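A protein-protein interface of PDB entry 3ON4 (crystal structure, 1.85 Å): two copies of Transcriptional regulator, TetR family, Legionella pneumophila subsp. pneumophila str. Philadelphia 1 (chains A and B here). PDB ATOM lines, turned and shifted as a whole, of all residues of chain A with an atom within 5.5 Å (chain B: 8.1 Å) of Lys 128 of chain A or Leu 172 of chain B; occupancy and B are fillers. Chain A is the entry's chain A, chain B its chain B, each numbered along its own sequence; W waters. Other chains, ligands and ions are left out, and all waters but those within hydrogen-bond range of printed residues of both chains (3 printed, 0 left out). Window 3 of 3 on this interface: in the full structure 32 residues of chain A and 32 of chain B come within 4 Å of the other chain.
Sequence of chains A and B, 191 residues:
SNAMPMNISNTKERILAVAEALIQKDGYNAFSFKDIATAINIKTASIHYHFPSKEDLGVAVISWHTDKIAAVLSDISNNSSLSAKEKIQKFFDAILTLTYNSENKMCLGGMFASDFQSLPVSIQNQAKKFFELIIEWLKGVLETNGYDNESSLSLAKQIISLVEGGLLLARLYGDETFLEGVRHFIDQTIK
O of Phe 116 of chain A is in hydrogen-bond range of NE2 of Gln 124 of chain A, 2.8 Å away.
O of Asn 104 of chain B is in hydrogen-bond range of NE of Arg 171 of chain B, 2.8 Å away.
Ala 113 of chain A touches Leu 168 of chain B.
O of Ala 113 of chain A touches NH1 of Arg 171 of chain B (3.9 Å).
Leu 172 of chain B touches Ala 113 of chain A (CD2 to O, 3.8 Å).
Phe 116 of chain A touches Leu 172 of chain B.
Lys 128 of chain A touches Leu 172 of chain B.
CD1 of Tyr 173 of chain B touches CD of Lys 128 of chain A (3.7 Å).
Leu 169 of chain B touches Phe 131 of chain A.
Of the printed residues of chain B, Phe 116 of chain A touches Leu 172 (3.6 Å).
Gln 124 of chain A touches none of the printed residues of chain B.
No residue of chain B comes within 4 Å of Ala 127 of chain A.
Of the printed residues of chain B, Lys 128 of chain A touches Leu 172 and Tyr 173.
Glu 132 of chain A touches none of the printed residues of chain B.
Of the printed residues of chain A, Leu 168 of chain B touches Ala 113 (3.8 Å).
Of the printed residues of chain A, Leu 169 of chain B touches Phe 131.
Printed residues of chain A within 4 Å of Arg 171 of chain B: Ala 113.
Of the printed residues of chain A, Leu 172 of chain B touches Ala 113, Phe 116 and Lys 128.
The nearest printed residue of chain B that does not touch Phe 116 of chain A is Arg 171 of chain B (4.8 Å).
Of the 13 printed residues of chain A, 4 touch a printed residue of chain B.
Hydrophobic or aromatic side chains of chain A within 4 Å of the printed part of chain B: Ala 113, Phe 116 and Phe 131.
Hydrophobic or aromatic side chains of chain B within 4 Å of the printed part of chain A: Leu 168, Leu 169, Leu 172 and Tyr 173.
Along chain B the printed residues that touch a printed residue of chain A span positions 168 to 173.
Among the printed residues, 7 pairs touch across the chains.
Among the printed residues, no Asp or Glu carboxylate lies within 4 Å of a Lys or Arg side-chain nitrogen of the other chain.
No position is printed for both chains.
Of the 7 pairs that touch across the chains among the printed residues, none has its exchanged pair printed and touching as well.
Water W1 bridges O of Leu 172 of chain B (2.7 Å) and NZ of Lys 128 of chain A (3.0 Å).
Water W2 lies within hydrogen-bond range of O of Ala 113 of chain A, O of Leu 168 of chain B and NH1 of Arg 171 of chain B.
Water W3 bridges the guanidinium group (NH1) of Arg 171 of chain B (2.9 Å) and the backbone NH (N) of Phe 116 of chain A (3.2 Å).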
ATOM      1  N   ALA A 113       1.188  -4.532  23.541  1.00  0.00           N
ATOM      2  CA  ALA A 113      -0.002  -4.111  22.798  1.00  0.00           C
ATOM      3  C   ALA A 113      -0.707  -5.279  22.120  1.00  0.00           C
ATOM      4  O   ALA A 113      -1.927  -5.349  22.157  1.00  0.00           O
ATOM      5  CB  ALA A 113       0.325  -3.027  21.769  1.00  0.00           C
ATOM      6  N   PHE A 116      -2.537  -7.366  24.728  1.00  0.00           N
ATOM      7  CA  PHE A 116      -3.215  -6.456  25.688  1.00  0.00           C
ATOM      8  C   PHE A 116      -4.426  -7.052  26.393  1.00  0.00           C
ATOM      9  O   PHE A 116      -4.535  -6.975  27.631  1.00  0.00           O
ATOM     10  CB  PHE A 116      -3.580  -5.169  24.952  1.00  0.00           C
ATOM     11  CG  PHE A 116      -3.885  -4.010  25.843  1.00  0.00           C
ATOM     12  CD1 PHE A 116      -2.858  -3.203  26.315  1.00  0.00           C
ATOM     13  CD2 PHE A 116      -5.187  -3.695  26.168  1.00  0.00           C
ATOM     14  CE1 PHE A 116      -3.131  -2.108  27.098  1.00  0.00           C
ATOM     15  CE2 PHE A 116      -5.471  -2.601  26.976  1.00  0.00           C
ATOM     16  CZ  PHE A 116      -4.431  -1.803  27.427  1.00  0.00           C
ATOM     17  N   ILE A 123      -0.520  -4.243  33.994  1.00  0.00           N
ATOM     18  CA  ILE A 123       0.416  -4.270  32.877  1.00  0.00           C
ATOM     19  C   ILE A 123      -0.134  -3.442  31.716  1.00  0.00           C
ATOM     20  O   ILE A 123       0.611  -2.707  31.045  1.00  0.00           O
ATOM     21  CB  ILE A 123       0.731  -5.717  32.456  1.00  0.00           C
ATOM     22  CG1 ILE A 123       1.404  -6.465  33.635  1.00  0.00           C
ATOM     23  CG2 ILE A 123       1.629  -5.756  31.254  1.00  0.00           C
ATOM     24  CD1 ILE A 123       1.711  -7.940  33.316  1.00  0.00           C
ATOM     25  N   GLN A 124      -1.426  -3.593  31.454  1.00  0.00           N
ATOM     26  CA  GLN A 124      -2.115  -2.762  30.463  1.00  0.00           C
ATOM     27  C   GLN A 124      -1.811  -1.279  30.673  1.00  0.00           C
ATOM     28  O   GLN A 124      -1.444  -0.572  29.734  1.00  0.00           O
ATOM     29  CB  GLN A 124      -3.633  -2.973  30.542  1.00  0.00           C
ATOM     30  CG  GLN A 124      -4.111  -4.315  30.032  1.00  0.00           C
ATOM     31  CD  GLN A 124      -5.619  -4.432  30.059  1.00  0.00           C
ATOM     32  OE1 GLN A 124      -6.293  -3.704  30.787  1.00  0.00           O
ATOM     33  NE2 GLN A 124      -6.149  -5.359  29.300  1.00  0.00           N
ATOM     34  N   ASN A 125      -1.977  -0.817  31.909  1.00  0.00           N
ATOM     35  CA  ASN A 125      -1.745   0.587  32.250  1.00  0.00           C
ATOM     36  C   ASN A 125      -0.269   1.016  32.043  1.00  0.00           C
ATOM     37  O   ASN A 125       0.009   2.116  31.551  1.00  0.00           O
ATOM     38  CB  ASN A 125      -2.281   0.906  33.665  1.00  0.00           C
ATOM     39  CG  ASN A 125      -3.814   0.894  33.722  1.00  0.00           C
ATOM     40  OD1 ASN A 125      -4.484   0.670  32.709  1.00  0.00           O
ATOM     41  ND2 ASN A 125      -4.368   1.117  34.900  1.00  0.00           N
ATOM     42  N   GLN A 126       0.679   0.130  32.327  1.00  0.00           N
ATOM     43  CA  GLN A 126       2.090   0.462  32.065  1.00  0.00           C
ATOM     44  C   GLN A 126       2.372   0.523  30.569  1.00  0.00           C
ATOM     45  O   GLN A 126       3.120   1.391  30.092  1.00  0.00           O
ATOM     46  CB  GLN A 126       3.038  -0.542  32.717  1.00  0.00           C
ATOM     47  CG  GLN A 126       2.994  -0.554  34.199  1.00  0.00           C
ATOM     48  CD  GLN A 126       3.576   0.693  34.846  1.00  0.00           C
ATOM     49  OE1 GLN A 126       4.443   1.378  34.280  1.00  0.00           O
ATOM     50  NE2 GLN A 126       3.088   1.000  36.036  1.00  0.00           N
ATOM     51  N   ALA A 127       1.791  -0.405  29.815  1.00  0.00           N
ATOM     52  CA  ALA A 127       1.926  -0.376  28.353  1.00  0.00           C
ATOM     53  C   ALA A 127       1.370   0.910  27.744  1.00  0.00           C
ATOM     54  O   ALA A 127       2.000   1.513  26.855  1.00  0.00           O
ATOM     55  CB  ALA A 127       1.245  -1.623  27.714  1.00  0.00           C
ATOM     56  N   LYS A 128       0.210   1.363  28.221  1.00  0.00           N
ATOM     57  CA  LYS A 128      -0.356   2.627  27.736  1.00  0.00           C
ATOM     58  C   LYS A 128       0.568   3.808  28.053  1.00  0.00           C
ATOM     59  O   LYS A 128       0.720   4.724  27.230  1.00  0.00           O
ATOM     60  CB  LYS A 128      -1.770   2.856  28.295  1.00  0.00           C
ATOM     61  CG  LYS A 128      -2.779   1.937  27.650  1.00  0.00           C
ATOM     62  CD  LYS A 128      -4.223   2.291  27.972  1.00  0.00           C
ATOM     63  CE  LYS A 128      -4.659   1.749  29.308  1.00  0.00           C
ATOM     64  NZ  LYS A 128      -5.994   2.300  29.723  1.00  0.00           N
ATOM     65  N   LYS A 129       1.183   3.770  29.232  1.00  0.00           N
ATOM     66  CA  LYS A 129       2.125   4.801  29.653  1.00  0.00           C
ATOM     67  C   LYS A 129       3.319   4.903  28.719  1.00  0.00           C
ATOM     68  O   LYS A 129       3.766   6.005  28.401  1.00  0.00           O
ATOM     69  CB  LYS A 129       2.624   4.547  31.073  1.00  0.00           C
ATOM     70  CG  LYS A 129       1.708   4.994  32.158  1.00  0.00           C
ATOM     71  CD  LYS A 129       2.439   4.967  33.500  1.00  0.00           C
ATOM     72  CE  LYS A 129       3.381   6.166  33.661  1.00  0.00           C
ATOM     73  NZ  LYS A 129       4.093   6.192  34.984  1.00  0.00           N
ATOM     74  N   PHE A 130       3.810   3.757  28.255  1.00  0.00           N
ATOM     75  CA  PHE A 130       4.913   3.678  27.277  1.00  0.00           C
ATOM     76  C   PHE A 130       4.571   4.414  25.982  1.00  0.00           C
ATOM     77  O   PHE A 130       5.331   5.283  25.525  1.00  0.00           O
ATOM     78  CB  PHE A 130       5.263   2.214  26.994  1.00  0.00           C
ATOM     79  CG  PHE A 130       6.290   1.995  25.896  1.00  0.00           C
ATOM     80  CD1 PHE A 130       7.642   2.068  26.164  1.00  0.00           C
ATOM     81  CD2 PHE A 130       5.894   1.719  24.593  1.00  0.00           C
ATOM     82  CE1 PHE A 130       8.587   1.852  25.173  1.00  0.00           C
ATOM     83  CE2 PHE A 130       6.841   1.518  23.579  1.00  0.00           C
ATOM     84  CZ  PHE A 130       8.190   1.567  23.878  1.00  0.00           C
ATOM     85  N   PHE A 131       3.417   4.094  25.403  1.00  0.00           N
ATOM     86  CA  PHE A 131       3.009   4.762  24.171  1.00  0.00           C
ATOM     87  C   PHE A 131       2.714   6.252  24.358  1.00  0.00           C
ATOM     88  O   PHE A 131       3.083   7.065  23.511  1.00  0.00           O
ATOM     89  CB  PHE A 131       1.864   4.010  23.498  1.00  0.00           C
ATOM     90  CG  PHE A 131       2.337   2.734  22.851  1.00  0.00           C
ATOM     91  CD1 PHE A 131       3.185   2.790  21.756  1.00  0.00           C
ATOM     92  CD2 PHE A 131       2.025   1.491  23.392  1.00  0.00           C
ATOM     93  CE1 PHE A 131       3.684   1.630  21.186  1.00  0.00           C
ATOM     94  CE2 PHE A 131       2.512   0.338  22.817  1.00  0.00           C
ATOM     95  CZ  PHE A 131       3.345   0.403  21.720  1.00  0.00           C
ATOM     96  N   GLU A 132       2.065   6.597  25.465  1.00  0.00           N
ATOM     97  CA  GLU A 132       1.787   7.994  25.787  1.00  0.00           C
ATOM     98  C   GLU A 132       3.088   8.798  25.855  1.00  0.00           C
ATOM     99  O   GLU A 132       3.140   9.906  25.347  1.00  0.00           O
ATOM    100  CB  GLU A 132       0.991   8.093  27.108  1.00  0.00           C
ATOM    101  CG  GLU A 132      -0.462   7.674  26.891  1.00  0.00           C
ATOM    102  CD  GLU A 132      -1.214   7.332  28.165  1.00  0.00           C
ATOM    103  OE1 GLU A 132      -0.707   7.631  29.276  1.00  0.00           O
ATOM    104  OE2 GLU A 132      -2.331   6.754  28.030  1.00  0.00           O
ATOM    105  N   LEU A 133       4.139   8.226  26.438  1.00  0.00           N
ATOM    106  CA  LEU A 133       5.432   8.897  26.522  1.00  0.00           C
ATOM    107  C   LEU A 133       6.052   9.114  25.139  1.00  0.00           C
ATOM    108  O   LEU A 133       6.539  10.198  24.843  1.00  0.00           O
ATOM    109  CB  LEU A 133       6.395   8.100  27.381  1.00  0.00           C
ATOM    110  CG  LEU A 133       7.728   8.792  27.675  1.00  0.00           C
ATOM    111  CD1 LEU A 133       8.125   8.605  29.148  1.00  0.00           C
ATOM    112  CD2 LEU A 133       8.774   8.258  26.735  1.00  0.00           C
ATOM    113  N   TYR B 100     -11.140  -3.787  14.267  1.00  0.00           N
ATOM    114  CA  TYR B 100     -11.580  -2.763  15.214  1.00  0.00           C
ATOM    115  C   TYR B 100     -13.089  -2.735  15.431  1.00  0.00           C
ATOM    116  O   TYR B 100     -13.555  -2.665  16.577  1.00  0.00           O
ATOM    117  CB  TYR B 100     -11.077  -1.383  14.755  1.00  0.00           C
ATOM    118  CG  TYR B 100     -11.378  -0.242  15.694  1.00  0.00           C
ATOM    119  CD1 TYR B 100     -10.515   0.090  16.752  1.00  0.00           C
ATOM    120  CD2 TYR B 100     -12.523   0.542  15.507  1.00  0.00           C
ATOM    121  CE1 TYR B 100     -10.801   1.168  17.596  1.00  0.00           C
ATOM    122  CE2 TYR B 100     -12.815   1.612  16.343  1.00  0.00           C
ATOM    123  CZ  TYR B 100     -11.942   1.934  17.373  1.00  0.00           C
ATOM    124  OH  TYR B 100     -12.282   2.989  18.182  1.00  0.00           O
ATOM    125  N   ASN B 104     -13.471  -4.938  18.862  1.00  0.00           N
ATOM    126  CA  ASN B 104     -12.133  -4.363  19.148  1.00  0.00           C
ATOM    127  C   ASN B 104     -10.987  -5.329  18.858  1.00  0.00           C
ATOM    128  O   ASN B 104      -9.985  -5.315  19.549  1.00  0.00           O
ATOM    129  CB  ASN B 104     -12.039  -3.930  20.612  1.00  0.00           C
ATOM    130  CG  ASN B 104     -10.898  -2.951  20.852  1.00  0.00           C
ATOM    131  OD1 ASN B 104     -10.724  -2.010  20.084  1.00  0.00           O
ATOM    132  ND2 ASN B 104     -10.169  -3.134  21.942  1.00  0.00           N
ATOM    133  N   GLY B 165       0.097  -1.410  12.416  1.00  0.00           N
ATOM    134  CA  GLY B 165       0.431  -0.565  13.560  1.00  0.00           C
ATOM    135  C   GLY B 165      -0.731   0.286  14.064  1.00  0.00           C
ATOM    136  O   GLY B 165      -0.906   0.452  15.266  1.00  0.00           O
ATOM    137  N   GLY B 166      -1.524   0.825  13.147  1.00  0.00           N
ATOM    138  CA  GLY B 166      -2.687   1.650  13.470  1.00  0.00           C
ATOM    139  C   GLY B 166      -3.748   0.855  14.222  1.00  0.00           C
ATOM    140  O   GLY B 166      -4.304   1.307  15.219  1.00  0.00           O
ATOM    141  N   LEU B 167      -4.010  -0.356  13.750  1.00  0.00           N
ATOM    142  CA  LEU B 167      -4.946  -1.245  14.397  1.00  0.00           C
ATOM    143  C   LEU B 167      -4.444  -1.653  15.784  1.00  0.00           C
ATOM    144  O   LEU B 167      -5.206  -1.688  16.726  1.00  0.00           O
ATOM    145  CB  LEU B 167      -5.179  -2.494  13.541  1.00  0.00           C
ATOM    146  CG  LEU B 167      -5.974  -2.292  12.265  1.00  0.00           C
ATOM    147  CD1 LEU B 167      -5.923  -3.614  11.540  1.00  0.00           C
ATOM    148  CD2 LEU B 167      -7.419  -1.823  12.572  1.00  0.00           C
ATOM    149  N   LEU B 168      -3.160  -1.942  15.892  1.00  0.00           N
ATOM    150  CA  LEU B 168      -2.549  -2.330  17.140  1.00  0.00           C
ATOM    151  C   LEU B 168      -2.738  -1.297  18.251  1.00  0.00           C
ATOM    152  O   LEU B 168      -3.067  -1.638  19.387  1.00  0.00           O
ATOM    153  CB  LEU B 168      -1.044  -2.547  16.911  1.00  0.00           C
ATOM    154  CG  LEU B 168      -0.263  -3.156  18.054  1.00  0.00           C
ATOM    155  CD1 LEU B 168      -0.568  -4.655  18.190  1.00  0.00           C
ATOM    156  CD2 LEU B 168       1.223  -2.932  17.820  1.00  0.00           C
ATOM    157  N   LEU B 169      -2.522  -0.033  17.919  1.00  0.00           N
ATOM    158  CA  LEU B 169      -2.607   1.039  18.887  1.00  0.00           C
ATOM    159  C   LEU B 169      -4.019   1.576  19.074  1.00  0.00           C
ATOM    160  O   LEU B 169      -4.376   1.968  20.191  1.00  0.00           O
ATOM    161  CB  LEU B 169      -1.613   2.164  18.509  1.00  0.00           C
ATOM    162  CG  LEU B 169      -0.160   1.689  18.318  1.00  0.00           C
ATOM    163  CD1 LEU B 169       0.746   2.816  17.861  1.00  0.00           C
ATOM    164  CD2 LEU B 169       0.389   0.999  19.602  1.00  0.00           C
ATOM    165  N   ALA B 170      -4.842   1.608  18.024  1.00  0.00           N
ATOM    166  CA  ALA B 170      -6.222   2.128  18.166  1.00  0.00           C
ATOM    167  C   ALA B 170      -7.035   1.342  19.196  1.00  0.00           C
ATOM    168  O   ALA B 170      -7.834   1.929  19.931  1.00  0.00           O
ATOM    169  CB  ALA B 170      -6.971   2.073  16.834  1.00  0.00           C
ATOM    170  N   ARG B 171      -6.812   0.026  19.240  1.00  0.00           N
ATOM    171  CA  ARG B 171      -7.584  -0.893  20.101  1.00  0.00           C
ATOM    172  C   ARG B 171      -7.178  -0.864  21.593  1.00  0.00           C
ATOM    173  O   ARG B 171      -7.867  -1.417  22.448  1.00  0.00           O
ATOM    174  CB  ARG B 171      -7.550  -2.307  19.493  1.00  0.00           C
ATOM    175  CG  ARG B 171      -6.237  -2.989  19.583  1.00  0.00           C
ATOM    176  CD  ARG B 171      -6.298  -4.330  18.849  1.00  0.00           C
ATOM    177  NE  ARG B 171      -7.152  -5.288  19.529  1.00  0.00           N
ATOM    178  CZ  ARG B 171      -6.737  -6.234  20.379  1.00  0.00           C
ATOM    179  NH1 ARG B 171      -5.455  -6.341  20.709  1.00  0.00           N
ATOM    180  NH2 ARG B 171      -7.622  -7.055  20.927  1.00  0.00           N
ATOM    181  N   LEU B 172      -6.114  -0.141  21.931  1.00  0.00           N
ATOM    182  CA  LEU B 172      -5.696  -0.029  23.324  1.00  0.00           C
ATOM    183  C   LEU B 172      -6.552   0.907  24.155  1.00  0.00           C
ATOM    184  O   LEU B 172      -6.760   0.664  25.343  1.00  0.00           O
ATOM    185  CB  LEU B 172      -4.245   0.447  23.437  1.00  0.00           C
ATOM    186  CG  LEU B 172      -3.230  -0.393  22.678  1.00  0.00           C
ATOM    187  CD1 LEU B 172      -1.821   0.127  23.013  1.00  0.00           C
ATOM    188  CD2 LEU B 172      -3.391  -1.911  22.987  1.00  0.00           C
ATOM    189  N   TYR B 173      -7.061   1.975  23.573  1.00  0.00           N
ATOM    190  CA  TYR B 173      -7.953   2.822  24.347  1.00  0.00           C
ATOM    191  C   TYR B 173      -8.949   3.561  23.446  1.00  0.00           C
ATOM    192  O   TYR B 173      -9.422   4.658  23.772  1.00  0.00           O
ATOM    193  CB  TYR B 173      -7.149   3.739  25.309  1.00  0.00           C
ATOM    194  CG  TYR B 173      -5.943   4.406  24.694  1.00  0.00           C
ATOM    195  CD1 TYR B 173      -4.714   3.741  24.639  1.00  0.00           C
ATOM    196  CD2 TYR B 173      -6.020   5.698  24.165  1.00  0.00           C
ATOM    197  CE1 TYR B 173      -3.605   4.332  24.062  1.00  0.00           C
ATOM    198  CE2 TYR B 173      -4.911   6.300  23.580  1.00  0.00           C
ATOM    199  CZ  TYR B 173      -3.700   5.605  23.532  1.00  0.00           C
ATOM    200  OH  TYR B 173      -2.567   6.168  22.967  1.00  0.00           O
ATOM    201  N   GLY B 174      -9.313   2.927  22.335  1.00  0.00           N
ATOM    202  CA  GLY B 174     -10.388   3.440  21.493  1.00  0.00           C
ATOM    203  C   GLY B 174     -10.004   4.751  20.822  1.00  0.00           C
ATOM    204  O   GLY B 174     -10.884   5.601  20.594  1.00  0.00           O
ATOM    205  N   ASP B 175      -8.703   4.967  20.538  1.00  0.00           N
ATOM    206  CA  ASP B 175      -8.302   6.237  19.877  1.00  0.00           C
ATOM    207  C   ASP B 175      -8.442   6.075  18.352  1.00  0.00           C
ATOM    208  O   ASP B 175      -7.598   5.490  17.686  1.00  0.00           O
ATOM    209  CB  ASP B 175      -6.898   6.697  20.297  1.00  0.00           C
ATOM    210  CG  ASP B 175      -6.549   8.067  19.773  1.00  0.00           C
ATOM    211  OD1 ASP B 175      -7.287   8.618  18.934  1.00  0.00           O
ATOM    212  OD2 ASP B 175      -5.517   8.606  20.196  1.00  0.00           O
ATOM    213  N   PHE B 178      -5.688   7.003  15.396  1.00  0.00           N
ATOM    214  CA  PHE B 178      -4.695   6.074  14.858  1.00  0.00           C
ATOM    215  C   PHE B 178      -5.158   5.519  13.509  1.00  0.00           C
ATOM    216  O   PHE B 178      -4.366   5.402  12.561  1.00  0.00           O
ATOM    217  CB  PHE B 178      -4.435   4.917  15.805  1.00  0.00           C
ATOM    218  CG  PHE B 178      -3.608   5.284  17.013  1.00  0.00           C
ATOM    219  CD1 PHE B 178      -2.243   5.486  16.911  1.00  0.00           C
ATOM    220  CD2 PHE B 178      -4.206   5.441  18.244  1.00  0.00           C
ATOM    221  CE1 PHE B 178      -1.505   5.845  18.019  1.00  0.00           C
ATOM    222  CE2 PHE B 178      -3.466   5.766  19.377  1.00  0.00           C
ATOM    223  CZ  PHE B 178      -2.113   5.963  19.262  1.00  0.00           C
HETATM  224  O   HOH W   1      -7.806   0.865  27.865  1.00  0.00           O
HETATM  225  O   HOH W   2      -3.526  -4.243  20.222  1.00  0.00           O
HETATM  226  O   HOH W   3      -4.894  -8.348  22.764  1.00  0.00           O
